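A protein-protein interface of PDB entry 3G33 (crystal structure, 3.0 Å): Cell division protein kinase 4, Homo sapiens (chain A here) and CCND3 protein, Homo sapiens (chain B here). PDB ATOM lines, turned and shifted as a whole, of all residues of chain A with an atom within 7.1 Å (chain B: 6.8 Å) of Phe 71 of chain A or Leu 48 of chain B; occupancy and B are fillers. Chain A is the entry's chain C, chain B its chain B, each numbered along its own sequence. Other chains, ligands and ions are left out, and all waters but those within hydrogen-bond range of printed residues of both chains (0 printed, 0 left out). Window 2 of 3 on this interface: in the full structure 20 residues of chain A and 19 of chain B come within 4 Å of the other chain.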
ATOM      1  N   LEU A  64       5.876  15.412  -9.390  1.00  0.00           N
ATOM      2  CA  LEU A  64       6.801  14.728 -10.283  1.00  0.00           C
ATOM      3  C   LEU A  64       6.255  14.716 -11.705  1.00  0.00           C
ATOM      4  O   LEU A  64       7.011  14.831 -12.670  1.00  0.00           O
ATOM      5  CB  LEU A  64       7.053  13.298  -9.806  1.00  0.00           C
ATOM      6  CG  LEU A  64       8.128  12.515 -10.564  1.00  0.00           C
ATOM      7  CD1 LEU A  64       9.478  13.205 -10.440  1.00  0.00           C
ATOM      8  CD2 LEU A  64       8.207  11.082 -10.062  1.00  0.00           C
ATOM      9  N   ARG A  66       3.950  17.009 -12.967  1.00  0.00           N
ATOM     10  CA  ARG A  66       3.993  18.388 -13.439  1.00  0.00           C
ATOM     11  C   ARG A  66       5.374  18.719 -13.996  1.00  0.00           C
ATOM     12  O   ARG A  66       5.500  19.436 -14.988  1.00  0.00           O
ATOM     13  CB  ARG A  66       3.634  19.359 -12.312  1.00  0.00           C
ATOM     14  CG  ARG A  66       2.215  19.211 -11.786  1.00  0.00           C
ATOM     15  CD  ARG A  66       1.187  19.808 -12.738  1.00  0.00           C
ATOM     16  NE  ARG A  66       1.316  21.258 -12.852  1.00  0.00           N
ATOM     17  CZ  ARG A  66       1.610  21.899 -13.979  1.00  0.00           C
ATOM     18  NH1 ARG A  66       1.796  21.218 -15.103  1.00  0.00           N
ATOM     19  NH2 ARG A  66       1.708  23.222 -13.987  1.00  0.00           N
ATOM     20  N   ARG A  67       6.408  18.187 -13.351  1.00  0.00           N
ATOM     21  CA  ARG A  67       7.784  18.437 -13.766  1.00  0.00           C
ATOM     22  C   ARG A  67       8.036  17.925 -15.181  1.00  0.00           C
ATOM     23  O   ARG A  67       8.688  18.593 -15.982  1.00  0.00           O
ATOM     24  CB  ARG A  67       8.762  17.784 -12.788  1.00  0.00           C
ATOM     25  CG  ARG A  67      10.204  18.243 -12.941  1.00  0.00           C
ATOM     26  CD  ARG A  67      11.107  17.545 -11.936  1.00  0.00           C
ATOM     27  NE  ARG A  67      12.451  18.113 -11.919  1.00  0.00           N
ATOM     28  CZ  ARG A  67      13.436  17.673 -11.143  1.00  0.00           C
ATOM     29  NH1 ARG A  67      13.228  16.655 -10.320  1.00  0.00           N
ATOM     30  NH2 ARG A  67      14.631  18.249 -11.192  1.00  0.00           N
ATOM     31  N   LEU A  68       7.514  16.740 -15.484  1.00  0.00           N
ATOM     32  CA  LEU A  68       7.678  16.153 -16.811  1.00  0.00           C
ATOM     33  C   LEU A  68       7.128  17.057 -17.907  1.00  0.00           C
ATOM     34  O   LEU A  68       7.743  17.212 -18.961  1.00  0.00           O
ATOM     35  CB  LEU A  68       7.012  14.778 -16.888  1.00  0.00           C
ATOM     36  CG  LEU A  68       7.911  13.569 -16.628  1.00  0.00           C
ATOM     37  CD1 LEU A  68       8.566  13.663 -15.258  1.00  0.00           C
ATOM     38  CD2 LEU A  68       7.119  12.278 -16.763  1.00  0.00           C
ATOM     39  N   GLU A  69       5.966  17.650 -17.658  1.00  0.00           N
ATOM     40  CA  GLU A  69       5.351  18.531 -18.640  1.00  0.00           C
ATOM     41  C   GLU A  69       6.376  19.520 -19.179  1.00  0.00           C
ATOM     42  O   GLU A  69       6.350  19.875 -20.357  1.00  0.00           O
ATOM     43  CB  GLU A  69       4.179  19.294 -18.028  1.00  0.00           C
ATOM     44  CG  GLU A  69       3.493  20.220 -19.012  1.00  0.00           C
ATOM     45  CD  GLU A  69       3.141  21.560 -18.402  1.00  0.00           C
ATOM     46  OE1 GLU A  69       2.952  21.626 -17.171  1.00  0.00           O
ATOM     47  OE2 GLU A  69       3.061  22.551 -19.159  1.00  0.00           O
ATOM     48  N   ALA A  70       7.277  19.962 -18.308  1.00  0.00           N
ATOM     49  CA  ALA A  70       8.285  20.950 -18.675  1.00  0.00           C
ATOM     50  C   ALA A  70       9.131  20.489 -19.856  1.00  0.00           C
ATOM     51  O   ALA A  70       9.387  21.255 -20.784  1.00  0.00           O
ATOM     52  CB  ALA A  70       9.170  21.277 -17.481  1.00  0.00           C
ATOM     53  N   PHE A  71       9.566  19.234 -19.816  1.00  0.00           N
ATOM     54  CA  PHE A  71      10.398  18.682 -20.878  1.00  0.00           C
ATOM     55  C   PHE A  71       9.657  18.659 -22.210  1.00  0.00           C
ATOM     56  O   PHE A  71      10.274  18.669 -23.275  1.00  0.00           O
ATOM     57  CB  PHE A  71      10.872  17.274 -20.514  1.00  0.00           C
ATOM     58  CG  PHE A  71      11.793  17.234 -19.330  1.00  0.00           C
ATOM     59  CD1 PHE A  71      13.144  17.496 -19.480  1.00  0.00           C
ATOM     60  CD2 PHE A  71      11.309  16.934 -18.069  1.00  0.00           C
ATOM     61  CE1 PHE A  71      13.995  17.460 -18.393  1.00  0.00           C
ATOM     62  CE2 PHE A  71      12.157  16.897 -16.978  1.00  0.00           C
ATOM     63  CZ  PHE A  71      13.502  17.160 -17.141  1.00  0.00           C
ATOM     64  N   GLU A  72       8.331  18.626 -22.143  1.00  0.00           N
ATOM     65  CA  GLU A  72       7.503  18.626 -23.343  1.00  0.00           C
ATOM     66  C   GLU A  72       7.914  17.537 -24.329  1.00  0.00           C
ATOM     67  O   GLU A  72       8.161  17.814 -25.502  1.00  0.00           O
ATOM     68  CB  GLU A  72       7.541  19.996 -24.025  1.00  0.00           C
ATOM     69  CG  GLU A  72       6.659  21.044 -23.365  1.00  0.00           C
ATOM     70  CD  GLU A  72       6.675  22.368 -24.106  1.00  0.00           C
ATOM     71  OE1 GLU A  72       7.778  22.905 -24.340  1.00  0.00           O
ATOM     72  OE2 GLU A  72       5.584  22.874 -24.449  1.00  0.00           O
ATOM     73  N   HIS A  73       7.986  16.300 -23.849  1.00  0.00           N
ATOM     74  CA  HIS A  73       8.266  15.165 -24.719  1.00  0.00           C
ATOM     75  C   HIS A  73       7.028  14.863 -25.559  1.00  0.00           C
ATOM     76  O   HIS A  73       5.912  14.850 -25.043  1.00  0.00           O
ATOM     77  CB  HIS A  73       8.665  13.940 -23.895  1.00  0.00           C
ATOM     78  CG  HIS A  73       9.376  12.886 -24.686  1.00  0.00           C
ATOM     79  ND1 HIS A  73       8.711  11.918 -25.405  1.00  0.00           N
ATOM     80  CD2 HIS A  73      10.697  12.648 -24.866  1.00  0.00           C
ATOM     81  CE1 HIS A  73       9.590  11.128 -25.997  1.00  0.00           C
ATOM     82  NE2 HIS A  73      10.803  11.550 -25.686  1.00  0.00           N
ATOM     83  N   PRO A  74       7.226  14.619 -26.862  1.00  0.00           N
ATOM     84  CA  PRO A  74       6.123  14.451 -27.804  1.00  0.00           C
ATOM     85  C   PRO A  74       5.390  13.121 -27.651  1.00  0.00           C
ATOM     86  O   PRO A  74       4.336  12.928 -28.256  1.00  0.00           O
ATOM     87  CB  PRO A  74       6.813  14.506 -29.176  1.00  0.00           C
ATOM     88  CG  PRO A  74       8.233  14.932 -28.912  1.00  0.00           C
ATOM     89  CD  PRO A  74       8.535  14.502 -27.522  1.00  0.00           C
ATOM     90  N   PHE A 135      12.032   7.782 -22.182  1.00  0.00           N
ATOM     91  CA  PHE A 135      11.967   9.073 -21.510  1.00  0.00           C
ATOM     92  C   PHE A 135      11.425   8.912 -20.093  1.00  0.00           C
ATOM     93  O   PHE A 135      11.970   9.473 -19.141  1.00  0.00           O
ATOM     94  CB  PHE A 135      11.095  10.045 -22.305  1.00  0.00           C
ATOM     95  CG  PHE A 135      10.776  11.314 -21.569  1.00  0.00           C
ATOM     96  CD1 PHE A 135      11.644  12.391 -21.611  1.00  0.00           C
ATOM     97  CD2 PHE A 135       9.608  11.430 -20.835  1.00  0.00           C
ATOM     98  CE1 PHE A 135      11.353  13.560 -20.934  1.00  0.00           C
ATOM     99  CE2 PHE A 135       9.312  12.595 -20.156  1.00  0.00           C
ATOM    100  CZ  PHE A 135      10.185  13.663 -20.205  1.00  0.00           C
ATOM    101  N   ASN A 139      13.426   9.419 -16.298  1.00  0.00           N
ATOM    102  CA  ASN A 139      12.965  10.267 -15.206  1.00  0.00           C
ATOM    103  C   ASN A 139      12.465   9.464 -14.008  1.00  0.00           C
ATOM    104  O   ASN A 139      11.737   9.980 -13.161  1.00  0.00           O
ATOM    105  CB  ASN A 139      11.878  11.226 -15.696  1.00  0.00           C
ATOM    106  CG  ASN A 139      12.429  12.316 -16.594  1.00  0.00           C
ATOM    107  OD1 ASN A 139      13.211  13.161 -16.157  1.00  0.00           O
ATOM    108  ND2 ASN A 139      12.017  12.307 -17.857  1.00  0.00           N
ATOM    109  N   GLN B  43      22.630  18.866 -18.043  1.00  0.00           N
ATOM    110  CA  GLN B  43      21.906  19.436 -19.173  1.00  0.00           C
ATOM    111  C   GLN B  43      20.423  19.604 -18.856  1.00  0.00           C
ATOM    112  O   GLN B  43      19.834  20.649 -19.134  1.00  0.00           O
ATOM    113  CB  GLN B  43      22.091  18.567 -20.420  1.00  0.00           C
ATOM    114  CG  GLN B  43      23.505  18.581 -20.977  1.00  0.00           C
ATOM    115  CD  GLN B  43      23.697  17.589 -22.109  1.00  0.00           C
ATOM    116  OE1 GLN B  43      23.074  16.529 -22.133  1.00  0.00           O
ATOM    117  NE2 GLN B  43      24.568  17.929 -23.053  1.00  0.00           N
ATOM    118  N   SER B  44      19.825  18.572 -18.269  1.00  0.00           N
ATOM    119  CA  SER B  44      18.405  18.606 -17.931  1.00  0.00           C
ATOM    120  C   SER B  44      18.115  19.615 -16.824  1.00  0.00           C
ATOM    121  O   SER B  44      17.193  20.423 -16.938  1.00  0.00           O
ATOM    122  CB  SER B  44      17.914  17.212 -17.529  1.00  0.00           C
ATOM    123  OG  SER B  44      18.733  16.655 -16.518  1.00  0.00           O
ATOM    124  N   LEU B  45      18.904  19.568 -15.756  1.00  0.00           N
ATOM    125  CA  LEU B  45      18.756  20.523 -14.664  1.00  0.00           C
ATOM    126  C   LEU B  45      18.757  21.952 -15.194  1.00  0.00           C
ATOM    127  O   LEU B  45      17.836  22.724 -14.927  1.00  0.00           O
ATOM    128  CB  LEU B  45      19.873  20.348 -13.633  1.00  0.00           C
ATOM    129  CG  LEU B  45      19.708  19.190 -12.647  1.00  0.00           C
ATOM    130  CD1 LEU B  45      20.879  19.144 -11.677  1.00  0.00           C
ATOM    131  CD2 LEU B  45      18.390  19.318 -11.895  1.00  0.00           C
ATOM    132  N   LEU B  46      19.798  22.298 -15.945  1.00  0.00           N
ATOM    133  CA  LEU B  46      19.901  23.622 -16.545  1.00  0.00           C
ATOM    134  C   LEU B  46      18.619  23.981 -17.287  1.00  0.00           C
ATOM    135  O   LEU B  46      18.049  25.052 -17.083  1.00  0.00           O
ATOM    136  CB  LEU B  46      21.096  23.690 -17.500  1.00  0.00           C
ATOM    137  CG  LEU B  46      22.491  23.708 -16.870  1.00  0.00           C
ATOM    138  CD1 LEU B  46      23.563  23.591 -17.941  1.00  0.00           C
ATOM    139  CD2 LEU B  46      22.690  24.968 -16.043  1.00  0.00           C
ATOM    140  N   ARG B  47      18.173  23.073 -18.149  1.00  0.00           N
ATOM    141  CA  ARG B  47      16.956  23.277 -18.930  1.00  0.00           C
ATOM    142  C   ARG B  47      15.778  23.750 -18.082  1.00  0.00           C
ATOM    143  O   ARG B  47      15.058  24.673 -18.462  1.00  0.00           O
ATOM    144  CB  ARG B  47      16.563  21.985 -19.650  1.00  0.00           C
ATOM    145  CG  ARG B  47      17.172  21.800 -21.030  1.00  0.00           C
ATOM    146  CD  ARG B  47      16.493  20.644 -21.753  1.00  0.00           C
ATOM    147  NE  ARG B  47      16.821  20.593 -23.175  1.00  0.00           N
ATOM    148  CZ  ARG B  47      16.223  19.789 -24.047  1.00  0.00           C
ATOM    149  NH1 ARG B  47      15.264  18.967 -23.643  1.00  0.00           N
ATOM    150  NH2 ARG B  47      16.582  19.805 -25.325  1.00  0.00           N
ATOM    151  N   LEU B  48      15.585  23.108 -16.934  1.00  0.00           N
ATOM    152  CA  LEU B  48      14.389  23.319 -16.119  1.00  0.00           C
ATOM    153  C   LEU B  48      14.337  24.669 -15.403  1.00  0.00           C
ATOM    154  O   LEU B  48      13.257  25.221 -15.195  1.00  0.00           O
ATOM    155  CB  LEU B  48      14.245  22.193 -15.090  1.00  0.00           C
ATOM    156  CG  LEU B  48      14.030  20.772 -15.614  1.00  0.00           C
ATOM    157  CD1 LEU B  48      14.073  19.772 -14.468  1.00  0.00           C
ATOM    158  CD2 LEU B  48      12.717  20.669 -16.373  1.00  0.00           C
ATOM    159  N   GLU B  49      15.498  25.192 -15.021  1.00  0.00           N
ATOM    160  CA  GLU B  49      15.563  26.391 -14.183  1.00  0.00           C
ATOM    161  C   GLU B  49      14.518  27.442 -14.544  1.00  0.00           C
ATOM    162  O   GLU B  49      13.837  27.980 -13.670  1.00  0.00           O
ATOM    163  CB  GLU B  49      16.950  27.029 -14.257  1.00  0.00           C
ATOM    164  CG  GLU B  49      18.105  26.051 -14.275  1.00  0.00           C
ATOM    165  CD  GLU B  49      19.442  26.760 -14.327  1.00  0.00           C
ATOM    166  OE1 GLU B  49      20.191  26.552 -15.306  1.00  0.00           O
ATOM    167  OE2 GLU B  49      19.738  27.541 -13.397  1.00  0.00           O
ATOM    168  N   GLU B  50      14.410  27.745 -15.832  1.00  0.00           N
ATOM    169  CA  GLU B  50      13.530  28.809 -16.292  1.00  0.00           C
ATOM    170  C   GLU B  50      12.116  28.661 -15.734  1.00  0.00           C
ATOM    171  O   GLU B  50      11.433  29.652 -15.482  1.00  0.00           O
ATOM    172  CB  GLU B  50      13.513  28.851 -17.822  1.00  0.00           C
ATOM    173  CG  GLU B  50      14.888  29.094 -18.439  1.00  0.00           C
ATOM    174  CD  GLU B  50      14.902  28.913 -19.950  1.00  0.00           C
ATOM    175  OE1 GLU B  50      14.096  28.111 -20.464  1.00  0.00           O
ATOM    176  OE2 GLU B  50      15.727  29.570 -20.622  1.00  0.00           O
ATOM    177  N   ARG B  51      11.694  27.418 -15.528  1.00  0.00           N
ATOM    178  CA  ARG B  51      10.331  27.123 -15.098  1.00  0.00           C
ATOM    179  C   ARG B  51      10.102  27.419 -13.621  1.00  0.00           C
ATOM    180  O   ARG B  51       8.978  27.704 -13.206  1.00  0.00           O
ATOM    181  CB  ARG B  51      10.000  25.660 -15.385  1.00  0.00           C
ATOM    182  CG  ARG B  51       8.589  25.259 -15.013  1.00  0.00           C
ATOM    183  CD  ARG B  51       8.403  23.759 -15.143  1.00  0.00           C
ATOM    184  NE  ARG B  51       7.002  23.374 -15.018  1.00  0.00           N
ATOM    185  CZ  ARG B  51       6.167  23.272 -16.045  1.00  0.00           C
ATOM    186  NH1 ARG B  51       6.595  23.526 -17.273  1.00  0.00           N
ATOM    187  NH2 ARG B  51       4.906  22.916 -15.847  1.00  0.00           N
ATOM    188  N   TYR B  52      11.168  27.348 -12.832  1.00  0.00           N
ATOM    189  CA  TYR B  52      11.061  27.551 -11.395  1.00  0.00           C
ATOM    190  C   TYR B  52      11.802  28.808 -10.961  1.00  0.00           C
ATOM    191  O   TYR B  52      12.433  28.849  -9.903  1.00  0.00           O
ATOM    192  CB  TYR B  52      11.569  26.319 -10.649  1.00  0.00           C
ATOM    193  CG  TYR B  52      10.898  25.041 -11.099  1.00  0.00           C
ATOM    194  CD1 TYR B  52      11.545  24.157 -11.950  1.00  0.00           C
ATOM    195  CD2 TYR B  52       9.612  24.727 -10.684  1.00  0.00           C
ATOM    196  CE1 TYR B  52      10.934  22.990 -12.367  1.00  0.00           C
ATOM    197  CE2 TYR B  52       8.992  23.564 -11.095  1.00  0.00           C
ATOM    198  CZ  TYR B  52       9.658  22.699 -11.936  1.00  0.00           C
ATOM    199  OH  TYR B  52       9.046  21.538 -12.348  1.00  0.00           O
ATOM    200  N   VAL B  53      11.721  29.833 -11.802  1.00  0.00           N
ATOM    201  CA  VAL B  53      12.209  31.157 -11.460  1.00  0.00           C
ATOM    202  C   VAL B  53      11.022  32.111 -11.465  1.00  0.00           C
ATOM    203  O   VAL B  53      10.386  32.309 -12.500  1.00  0.00           O
ATOM    204  CB  VAL B  53      13.266  31.652 -12.461  1.00  0.00           C
ATOM    205  CG1 VAL B  53      13.732  33.049 -12.085  1.00  0.00           C
ATOM    206  CG2 VAL B  53      14.441  30.691 -12.512  1.00  0.00           C
ATOM    207  N   ALA B 167       8.310  20.273  -7.543  1.00  0.00           N
ATOM    208  CA  ALA B 167       9.611  19.653  -7.770  1.00  0.00           C
ATOM    209  C   ALA B 167      10.546  20.640  -8.460  1.00  0.00           C
ATOM    210  O   ALA B 167      11.137  20.333  -9.494  1.00  0.00           O
ATOM    211  CB  ALA B 167       9.463  18.391  -8.600  1.00  0.00           C
ATOM    212  N   VAL B 169      13.673  23.250  -9.328  1.00  0.00           N
ATOM    213  CA  VAL B 169      15.127  23.228  -9.299  1.00  0.00           C
ATOM    214  C   VAL B 169      15.640  24.485  -8.610  1.00  0.00           C
ATOM    215  O   VAL B 169      15.392  25.598  -9.072  1.00  0.00           O
ATOM    216  CB  VAL B 169      15.715  23.157 -10.718  1.00  0.00           C
ATOM    217  CG1 VAL B 169      17.221  23.357 -10.681  1.00  0.00           C
ATOM    218  CG2 VAL B 169      15.363  21.830 -11.370  1.00  0.00           C
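NH2 of Arg 51 of chain B lies within salt-bridge range of OE1 of Glu 69 of chain A (2.7 Å).
The side-chain carboxylate (OE1) of Glu 69 of chain A is in salt-bridge range of the guanidinium group (NH1) of Arg 66 of chain A (2.4 Å).
Among the printed residues, merely in contact across the chains: Ala 70 of chain A with Arg 51 of chain B (3.4 Å), Arg 67 of chain A with Leu 48 of chain B (3.4 Å), Arg 67 of chain A with Ala 167 of chain B (3.5 Å), Arg 67 of chain A with Tyr 52 of chain B (3.5 Å), Arg 66 of chain A with Arg 51 of chain B (3.6 Å), Arg 67 of chain A with Val 169 of chain B (3.7 Å), Phe 71 of chain A with Leu 48 of chain B (3.7 Å), Ala 70 of chain A with Leu 48 of chain B (3.8 Å) and Arg 67 of chain A with Leu 45 of chain B (3.97 Å).
Of the printed residues of chain B, Arg 66 of chain A touches Arg 51.
Printed residues of chain B within 4 Å of Glu 69 of chain A: Arg 51.
Of chain B, only Leu 48 comes within 4 Å of Phe 71 of chain A.
Glu 72 of chain A touches none of the printed residues of chain B.
Of the printed residues of chain A, Arg 51 of chain B touches Arg 66, Glu 69 and Ala 70.
Printed residues of chain A within 4 Å of Ala 167 of chain B: Arg 67 (3.5 Å).
Of the printed residues of chain A, Val 169 of chain B touches Arg 67.
The nearest residue of chain A that does not touch Leu 48 of chain B is Leu 68 of chain A (6.6 Å).
The nearest printed residue of chain A that does not touch Leu 45 of chain B is Phe 71 of chain A (6.0 Å).
Of the 13 printed residues of chain B, 6 touch a printed residue of chain A.
Among the printed residues, 10 pairs touch across the chains.
Among the printed residues, Asp or Glu carboxylates within 4 Å of a Lys or Arg side-chain nitrogen of the other chain: Glu 69 of chain A with Arg 51 of chain B (2.7 Å).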
